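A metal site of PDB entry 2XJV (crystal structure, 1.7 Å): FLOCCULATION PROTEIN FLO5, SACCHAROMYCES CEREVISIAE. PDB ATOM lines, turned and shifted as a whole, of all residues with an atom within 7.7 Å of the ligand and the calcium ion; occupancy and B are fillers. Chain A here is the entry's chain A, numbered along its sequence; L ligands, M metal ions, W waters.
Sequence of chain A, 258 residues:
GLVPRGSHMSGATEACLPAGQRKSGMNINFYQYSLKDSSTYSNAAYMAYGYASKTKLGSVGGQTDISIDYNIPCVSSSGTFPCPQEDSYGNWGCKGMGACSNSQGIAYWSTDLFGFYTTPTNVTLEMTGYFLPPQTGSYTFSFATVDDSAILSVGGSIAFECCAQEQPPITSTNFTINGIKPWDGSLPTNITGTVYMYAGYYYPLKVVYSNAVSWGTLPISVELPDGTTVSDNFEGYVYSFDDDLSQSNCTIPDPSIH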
ATOM      1  N   LYS A  36      -9.326 -15.074  16.867  1.00  0.00           N
ATOM      2  CA  LYS A  36      -8.595 -16.252  16.374  1.00  0.00           C
ATOM      3  C   LYS A  36      -8.806 -16.558  14.887  1.00  0.00           C
ATOM      4  O   LYS A  36      -8.416 -17.619  14.409  1.00  0.00           O
ATOM      5  CB  LYS A  36      -8.814 -17.480  17.304  1.00  0.00           C
ATOM      6  CG  LYS A  36      -8.079 -17.292  18.660  1.00  0.00           C
ATOM      7  CD  LYS A  36      -8.240 -18.468  19.610  1.00  0.00           C
ATOM      8  CE  LYS A  36      -9.580 -18.415  20.304  1.00  0.00           C
ATOM      9  NZ  LYS A  36      -9.655 -19.421  21.407  1.00  0.00           N
ATOM     10  N   SER A  38      -7.307 -16.284  11.716  1.00  0.00           N
ATOM     11  CA  SER A  38      -5.978 -16.012  11.182  1.00  0.00           C
ATOM     12  C   SER A  38      -5.950 -16.083   9.663  1.00  0.00           C
ATOM     13  O   SER A  38      -4.869 -16.199   9.085  1.00  0.00           O
ATOM     14  CB  SER A  38      -4.934 -16.959  11.773  1.00  0.00           C
ATOM     15  OG  SER A  38      -5.267 -18.315  11.519  1.00  0.00           O
ATOM     16  N   TYR A  41      -7.635 -11.642   7.417  1.00  0.00           N
ATOM     17  CA  TYR A  41      -6.746 -10.484   7.229  1.00  0.00           C
ATOM     18  C   TYR A  41      -5.525 -10.741   6.331  1.00  0.00           C
ATOM     19  O   TYR A  41      -4.662  -9.881   6.202  1.00  0.00           O
ATOM     20  CB  TYR A  41      -6.315  -9.889   8.568  1.00  0.00           C
ATOM     21  CG  TYR A  41      -5.649 -10.815   9.555  1.00  0.00           C
ATOM     22  CD1 TYR A  41      -5.795 -10.596  10.929  1.00  0.00           C
ATOM     23  CD2 TYR A  41      -4.852 -11.907   9.149  1.00  0.00           C
ATOM     24  CE1 TYR A  41      -5.195 -11.410  11.858  1.00  0.00           C
ATOM     25  CE2 TYR A  41      -4.235 -12.735  10.085  1.00  0.00           C
ATOM     26  CZ  TYR A  41      -4.411 -12.467  11.450  1.00  0.00           C
ATOM     27  OH  TYR A  41      -3.825 -13.262  12.402  1.00  0.00           O
ATOM     28  N   TYR A  70      -0.650  -2.674  22.161  1.00  0.00           N
ATOM     29  CA  TYR A  70      -1.654  -3.229  23.055  1.00  0.00           C
ATOM     30  C   TYR A  70      -1.117  -4.496  23.736  1.00  0.00           C
ATOM     31  O   TYR A  70      -0.667  -5.423  23.073  1.00  0.00           O
ATOM     32  CB  TYR A  70      -2.991  -3.525  22.335  1.00  0.00           C
ATOM     33  CG  TYR A  70      -3.897  -4.381  23.190  1.00  0.00           C
ATOM     34  CD1 TYR A  70      -4.498  -3.868  24.330  1.00  0.00           C
ATOM     35  CD2 TYR A  70      -4.108  -5.739  22.879  1.00  0.00           C
ATOM     36  CE1 TYR A  70      -5.299  -4.635  25.141  1.00  0.00           C
ATOM     37  CE2 TYR A  70      -4.925  -6.533  23.694  1.00  0.00           C
ATOM     38  CZ  TYR A  70      -5.502  -5.965  24.824  1.00  0.00           C
ATOM     39  OH  TYR A  70      -6.278  -6.733  25.662  1.00  0.00           O
ATOM     40  N   ILE A  72      -2.024  -7.541  26.562  1.00  0.00           N
ATOM     41  CA  ILE A  72      -3.099  -8.210  27.291  1.00  0.00           C
ATOM     42  C   ILE A  72      -2.887  -8.174  28.802  1.00  0.00           C
ATOM     43  O   ILE A  72      -1.741  -8.033  29.265  1.00  0.00           O
ATOM     44  CB  ILE A  72      -3.304  -9.685  26.845  1.00  0.00           C
ATOM     45  CG1 ILE A  72      -1.986 -10.473  26.868  1.00  0.00           C
ATOM     46  CG2 ILE A  72      -3.992  -9.718  25.477  1.00  0.00           C
ATOM     47  CD1 ILE A  72      -2.180 -11.987  26.969  1.00  0.00           C
ATOM     48  N   GLN A  85       4.732  -8.110  25.880  1.00  0.00           N
ATOM     49  CA  GLN A  85       4.861  -9.487  25.377  1.00  0.00           C
ATOM     50  C   GLN A  85       6.247 -10.069  25.602  1.00  0.00           C
ATOM     51  O   GLN A  85       6.386 -11.260  25.849  1.00  0.00           O
ATOM     52  CB  GLN A  85       4.392  -9.663  23.920  1.00  0.00           C
ATOM     53  CG  GLN A  85       5.160  -8.876  22.872  1.00  0.00           C
ATOM     54  CD  GLN A  85       4.515  -7.551  22.565  1.00  0.00           C
ATOM     55  OE1 GLN A  85       4.365  -6.708  23.450  1.00  0.00           O
ATOM     56  NE2 GLN A  85       4.135  -7.354  21.320  1.00  0.00           N
ATOM     57  N   SER A  88       6.451 -11.844  28.868  1.00  0.00           N
ATOM     58  CA  SER A  88       5.655 -13.058  29.062  1.00  0.00           C
ATOM     59  C   SER A  88       6.558 -14.283  28.996  1.00  0.00           C
ATOM     60  O   SER A  88       7.560 -14.297  28.254  1.00  0.00           O
ATOM     61  CB  SER A  88       4.480 -13.149  28.077  1.00  0.00           C
ATOM     62  OG  SER A  88       4.939 -13.350  26.738  1.00  0.00           O
ATOM     63  N   GLN A 104      -4.571 -16.455  27.594  1.00  0.00           N
ATOM     64  CA  GLN A 104      -4.094 -15.587  26.508  1.00  0.00           C
ATOM     65  C   GLN A 104      -5.035 -15.579  25.303  1.00  0.00           C
ATOM     66  O   GLN A 104      -4.939 -14.706  24.435  1.00  0.00           O
ATOM     67  CB  GLN A 104      -2.704 -16.007  26.037  1.00  0.00           C
ATOM     68  CG  GLN A 104      -1.602 -15.843  27.070  1.00  0.00           C
ATOM     69  CD  GLN A 104      -0.208 -16.030  26.459  1.00  0.00           C
ATOM     70  OE1 GLN A 104      -0.052 -16.225  25.250  1.00  0.00           O
ATOM     71  NE2 GLN A 104       0.814 -15.962  27.298  1.00  0.00           N
ATOM     72  N   PRO A 120      -9.349  -4.976  21.761  1.00  0.00           N
ATOM     73  CA  PRO A 120      -8.098  -4.824  20.976  1.00  0.00           C
ATOM     74  C   PRO A 120      -7.462  -6.157  20.623  1.00  0.00           C
ATOM     75  O   PRO A 120      -6.621  -6.207  19.715  1.00  0.00           O
ATOM     76  CB  PRO A 120      -7.185  -4.016  21.908  1.00  0.00           C
ATOM     77  CG  PRO A 120      -8.134  -3.275  22.838  1.00  0.00           C
ATOM     78  CD  PRO A 120      -9.226  -4.342  23.090  1.00  0.00           C
ATOM     79  N   THR A 121      -7.875  -7.226  21.313  1.00  0.00           N
ATOM     80  CA  THR A 121      -7.483  -8.594  20.933  1.00  0.00           C
ATOM     81  C   THR A 121      -7.974  -9.023  19.555  1.00  0.00           C
ATOM     82  O   THR A 121      -7.373  -9.887  18.930  1.00  0.00           O
ATOM     83  CB  THR A 121      -8.061  -9.613  21.932  1.00  0.00           C
ATOM     84  OG1 THR A 121      -9.446  -9.340  22.137  1.00  0.00           O
ATOM     85  CG2 THR A 121      -7.334  -9.533  23.274  1.00  0.00           C
ATOM     86  N   ASN A 122      -9.101  -8.463  19.119  1.00  0.00           N
ATOM     87  CA  ASN A 122      -9.743  -8.875  17.870  1.00  0.00           C
ATOM     88  C   ASN A 122     -10.591  -7.726  17.331  1.00  0.00           C
ATOM     89  O   ASN A 122     -11.694  -7.445  17.813  1.00  0.00           O
ATOM     90  CB  ASN A 122     -10.556 -10.194  18.047  1.00  0.00           C
ATOM     91  CG  ASN A 122     -11.679 -10.063  19.069  1.00  0.00           C
ATOM     92  OD1 ASN A 122     -11.437  -9.890  20.281  1.00  0.00           O
ATOM     93  ND2 ASN A 122     -12.926 -10.149  18.587  1.00  0.00           N
ATOM     94  N   VAL A 146       4.782  -5.780  12.670  1.00  0.00           N
ATOM     95  CA  VAL A 146       3.318  -5.864  12.457  1.00  0.00           C
ATOM     96  C   VAL A 146       2.741  -7.090  13.196  1.00  0.00           C
ATOM     97  O   VAL A 146       3.157  -8.226  12.937  1.00  0.00           O
ATOM     98  CB  VAL A 146       2.958  -5.997  10.950  1.00  0.00           C
ATOM     99  CG1 VAL A 146       1.420  -6.044  10.763  1.00  0.00           C
ATOM    100  CG2 VAL A 146       3.586  -4.858  10.120  1.00  0.00           C
ATOM    101  N   ASP A 147       1.792  -6.853  14.100  1.00  0.00           N
ATOM    102  CA  ASP A 147       1.074  -7.953  14.759  1.00  0.00           C
ATOM    103  C   ASP A 147      -0.377  -7.458  14.874  1.00  0.00           C
ATOM    104  O   ASP A 147      -0.649  -6.648  15.751  1.00  0.00           O
ATOM    105  CB  ASP A 147       1.710  -8.239  16.153  1.00  0.00           C
ATOM    106  CG  ASP A 147       0.910  -9.265  16.995  1.00  0.00           C
ATOM    107  OD1 ASP A 147       1.473  -9.783  17.969  1.00  0.00           O
ATOM    108  OD2 ASP A 147      -0.266  -9.548  16.715  1.00  0.00           O
ATOM    109  N   ASP A 148      -1.326  -7.937  14.042  1.00  0.00           N
ATOM    110  CA  ASP A 148      -1.160  -9.084  13.141  1.00  0.00           C
ATOM    111  C   ASP A 148      -0.942  -8.741  11.664  1.00  0.00           C
ATOM    112  O   ASP A 148      -0.112  -9.341  10.986  1.00  0.00           O
ATOM    113  CB  ASP A 148      -2.386 -10.002  13.233  1.00  0.00           C
ATOM    114  CG  ASP A 148      -2.457 -10.805  14.535  1.00  0.00           C
ATOM    115  OD1 ASP A 148      -1.557 -10.691  15.386  1.00  0.00           O
ATOM    116  OD2 ASP A 148      -3.426 -11.566  14.697  1.00  0.00           O
ATOM    117  N   SER A 149      -1.724  -7.794  11.156  1.00  0.00           N
ATOM    118  CA  SER A 149      -1.774  -7.520   9.711  1.00  0.00           C
ATOM    119  C   SER A 149      -2.013  -6.037   9.507  1.00  0.00           C
ATOM    120  O   SER A 149      -2.788  -5.425  10.259  1.00  0.00           O
ATOM    121  CB  SER A 149      -2.919  -8.315   9.073  1.00  0.00           C
ATOM    122  OG  SER A 149      -2.825  -8.327   7.659  1.00  0.00           O
ATOM    123  N   LYS A 181      -0.317 -10.028   6.752  1.00  0.00           N
ATOM    124  CA  LYS A 181       0.167 -11.290   7.292  1.00  0.00           C
ATOM    125  C   LYS A 181       0.225 -12.339   6.177  1.00  0.00           C
ATOM    126  O   LYS A 181      -0.805 -12.669   5.582  1.00  0.00           O
ATOM    127  CB  LYS A 181      -0.743 -11.764   8.430  1.00  0.00           C
ATOM    128  CG  LYS A 181      -0.191 -12.945   9.228  1.00  0.00           C
ATOM    129  CD  LYS A 181      -0.462 -12.750  10.720  1.00  0.00           C
ATOM    130  CE  LYS A 181       0.232 -13.826  11.543  1.00  0.00           C
ATOM    131  NZ  LYS A 181       0.557 -13.332  12.917  1.00  0.00           N
ATOM    132  N   TYR A 209      -5.379  -1.666  10.076  1.00  0.00           N
ATOM    133  CA  TYR A 209      -4.680  -2.557  10.975  1.00  0.00           C
ATOM    134  C   TYR A 209      -5.642  -3.593  11.569  1.00  0.00           C
ATOM    135  O   TYR A 209      -6.784  -3.256  11.930  1.00  0.00           O
ATOM    136  CB  TYR A 209      -4.015  -1.744  12.103  1.00  0.00           C
ATOM    137  CG  TYR A 209      -3.673  -2.610  13.296  1.00  0.00           C
ATOM    138  CD1 TYR A 209      -2.461  -3.298  13.351  1.00  0.00           C
ATOM    139  CD2 TYR A 209      -4.579  -2.763  14.354  1.00  0.00           C
ATOM    140  CE1 TYR A 209      -2.148  -4.148  14.436  1.00  0.00           C
ATOM    141  CE2 TYR A 209      -4.277  -3.597  15.453  1.00  0.00           C
ATOM    142  CZ  TYR A 209      -3.067  -4.279  15.485  1.00  0.00           C
ATOM    143  OH  TYR A 209      -2.787  -5.103  16.555  1.00  0.00           O
ATOM    144  N   SER A 210      -5.172  -4.838  11.696  1.00  0.00           N
ATOM    145  CA  SER A 210      -5.996  -5.919  12.260  1.00  0.00           C
ATOM    146  C   SER A 210      -5.240  -6.740  13.302  1.00  0.00           C
ATOM    147  O   SER A 210      -4.026  -6.999  13.149  1.00  0.00           O
ATOM    148  CB  SER A 210      -6.534  -6.817  11.144  1.00  0.00           C
ATOM    149  OG  SER A 210      -7.561  -7.672  11.617  1.00  0.00           O
ATOM    150  N   ASN A 211      -5.958  -7.139  14.347  1.00  0.00           N
ATOM    151  CA  ASN A 211      -5.450  -8.081  15.355  1.00  0.00           C
ATOM    152  C   ASN A 211      -6.473  -9.209  15.513  1.00  0.00           C
ATOM    153  O   ASN A 211      -7.679  -8.951  15.529  1.00  0.00           O
ATOM    154  CB  ASN A 211      -5.239  -7.391  16.710  1.00  0.00           C
ATOM    155  CG  ASN A 211      -4.408  -8.257  17.687  1.00  0.00           C
ATOM    156  OD1 ASN A 211      -3.687  -9.161  17.273  1.00  0.00           O
ATOM    157  ND2 ASN A 211      -4.497  -7.948  18.964  1.00  0.00           N
ATOM    158  N   ALA A 212      -5.987 -10.460  15.581  1.00  0.00           N
ATOM    159  CA  ALA A 212      -6.837 -11.637  15.730  1.00  0.00           C
ATOM    160  C   ALA A 212      -6.779 -12.266  17.118  1.00  0.00           C
ATOM    161  O   ALA A 212      -7.750 -12.901  17.552  1.00  0.00           O
ATOM    162  CB  ALA A 212      -6.462 -12.692  14.691  1.00  0.00           C
ATOM    163  N   VAL A 213      -5.654 -12.111  17.807  1.00  0.00           N
ATOM    164  CA  VAL A 213      -5.526 -12.660  19.157  1.00  0.00           C
ATOM    165  C   VAL A 213      -4.486 -11.888  19.990  1.00  0.00           C
ATOM    166  O   VAL A 213      -3.511 -11.343  19.444  1.00  0.00           O
ATOM    167  CB  VAL A 213      -5.229 -14.189  19.132  1.00  0.00           C
ATOM    168  CG1 VAL A 213      -3.753 -14.466  18.833  1.00  0.00           C
ATOM    169  CG2 VAL A 213      -5.677 -14.858  20.477  1.00  0.00           C
ATOM    170  N   SER A 214      -4.733 -11.836  21.303  1.00  0.00           N
ATOM    171  CA  SER A 214      -3.793 -11.305  22.310  1.00  0.00           C
ATOM    172  C   SER A 214      -3.098  -9.980  21.923  1.00  0.00           C
ATOM    173  O   SER A 214      -3.788  -8.985  21.646  1.00  0.00           O
ATOM    174  CB  SER A 214      -2.774 -12.363  22.800  1.00  0.00           C
ATOM    175  OG  SER A 214      -1.941 -12.856  21.750  1.00  0.00           O
ATOM    176  N   TRP A 215      -1.763  -9.964  21.911  1.00  0.00           N
ATOM    177  CA  TRP A 215      -1.015  -8.710  21.695  1.00  0.00           C
ATOM    178  C   TRP A 215      -1.241  -8.132  20.303  1.00  0.00           C
ATOM    179  O   TRP A 215      -1.446  -8.867  19.325  1.00  0.00           O
ATOM    180  CB  TRP A 215       0.500  -8.924  21.920  1.00  0.00           C
ATOM    181  CG  TRP A 215       0.861  -9.110  23.381  1.00  0.00           C
ATOM    182  CD1 TRP A 215       1.208  -8.129  24.301  1.00  0.00           C
ATOM    183  CD2 TRP A 215       0.906 -10.353  24.089  1.00  0.00           C
ATOM    184  NE1 TRP A 215       1.470  -8.711  25.531  1.00  0.00           N
ATOM    185  CE2 TRP A 215       1.280 -10.068  25.439  1.00  0.00           C
ATOM    186  CE3 TRP A 215       0.651 -11.688  23.730  1.00  0.00           C
ATOM    187  CZ2 TRP A 215       1.426 -11.068  26.411  1.00  0.00           C
ATOM    188  CZ3 TRP A 215       0.804 -12.699  24.706  1.00  0.00           C
ATOM    189  CH2 TRP A 215       1.185 -12.371  26.024  1.00  0.00           C
ATOM    190  N   GLY A 216      -1.205  -6.810  20.242  1.00  0.00           N
ATOM    191  CA  GLY A 216      -1.296  -6.071  18.974  1.00  0.00           C
ATOM    192  C   GLY A 216      -0.201  -5.018  18.950  1.00  0.00           C
ATOM    193  O   GLY A 216       0.013  -4.297  19.924  1.00  0.00           O
ATOM    194  N   THR A 217       0.510  -4.932  17.823  1.00  0.00           N
ATOM    195  CA  THR A 217       1.644  -4.013  17.719  1.00  0.00           C
ATOM    196  C   THR A 217       1.779  -3.426  16.334  1.00  0.00           C
ATOM    197  O   THR A 217       1.794  -4.162  15.333  1.00  0.00           O
ATOM    198  CB  THR A 217       2.970  -4.700  18.110  1.00  0.00           C
ATOM    199  OG1 THR A 217       2.760  -5.495  19.280  1.00  0.00           O
ATOM    200  CG2 THR A 217       4.085  -3.659  18.339  1.00  0.00           C
HETATM  201  C1  LIG L   1       1.366 -13.325  19.355  1.00  0.00           C
HETATM  202  C2  LIG L   1      -0.046 -12.927  18.941  1.00  0.00           C
HETATM  203  C3  LIG L   1      -0.168 -13.186  17.440  1.00  0.00           C
HETATM  204  C4  LIG L   1       0.088 -14.681  17.183  1.00  0.00           C
HETATM  205  C5  LIG L   1       0.132 -14.993  15.694  1.00  0.00           C
HETATM  206  C6  LIG L   1       1.504 -14.822  19.134  1.00  0.00           C
HETATM  207  O1  LIG L   1       2.794 -15.201  19.577  1.00  0.00           O
HETATM  208  O2  LIG L   1       1.583 -12.989  20.696  1.00  0.00           O
HETATM  209  O3  LIG L   1      -0.286 -11.586  19.289  1.00  0.00           O
HETATM  210  O4  LIG L   1      -1.439 -12.796  16.977  1.00  0.00           O
HETATM  211  O5  LIG L   1       1.325 -15.122  17.760  1.00  0.00           O
HETATM  212  O6  LIG L   1      -1.006 -15.775  15.363  1.00  0.00           O
HETATM  213 CA    CA M   1      -1.858 -10.509  17.876  1.00  0.00          CA
HETATM  214  O   HOH W   1      -3.211 -14.235  14.873  1.00  0.00           O
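Water W1 lies within hydrogen-bond range of the side-chain carboxylate of Asp 148 (2.7 Å), the side-chain hydroxyl of Tyr 41 (2.7 Å) and an oxygen (O6) of the ligand (2.7 Å).
OH of Tyr 209 lies within hydrogen-bond range of O of Asp 147 (2.8 Å).
The backbone carbonyl oxygen of Asp 147 sits at hydrogen-bond distance from the backbone NH of Thr 217 (2.9 Å).
The side-chain amide nitrogen of Asn 211 is in hydrogen-bond range of the backbone carbonyl oxygen of Ser 214, at 3.0 Å.
O of Pro 120 lies within hydrogen-bond range of ND2 of Asn 211 (2.8 Å).
The backbone carbonyl oxygen (O) of Thr 121 lies within hydrogen-bond range of the backbone NH (N) of Val 213 (3.0 Å).
OD2 of Asp 148 sits at hydrogen-bond distance from N of Ala 212.
The side-chain carboxylate (OD2) of Asp 148 sits at hydrogen-bond distance from the side-chain hydroxyl (OH) of Tyr 41 (2.9 Å).
The side-chain hydroxyl of Ser 149 sits at hydrogen-bond distance from the backbone NH of Lys 181, 3.2 Å away.
NZ of Lys 181 touches C5 of the ligand, at 3.3 Å.
Hydrophobic or aromatic side chains within 4 Å of the ligand: Val 213 and Trp 215.
Within 4 Å of the ligand: Asp 147, Asp 148, Lys 181, Val 213, Ser 214 and Trp 215.
Along chain A the residues within 4 Å of the ligand span positions 147 to 215.
N of Trp 215 sits close to O3 of the ligand, 3.4 Å away.
The side-chain hydroxyl (OG) of Ser 214 sits close to an oxygen (O3) of the ligand (3.2 Å).
The calcium ion is bound by OD2 of Asp 147, 2.2 Å away.
O of Trp 215 binds the calcium ion (2.2 Å).
OD1 of Asn 211 is bound to the calcium ion, at 2.4 Å.
An oxygen (O3) of the ligand is bound to the calcium ion.
The calcium ion is bound by O of Val 213.
The calcium ion is bound by an oxygen (O4) of the ligand.
OD1 of Asp 148 binds the calcium ion (2.5 Å).
The calcium ion has seven donor atoms within binding distance.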
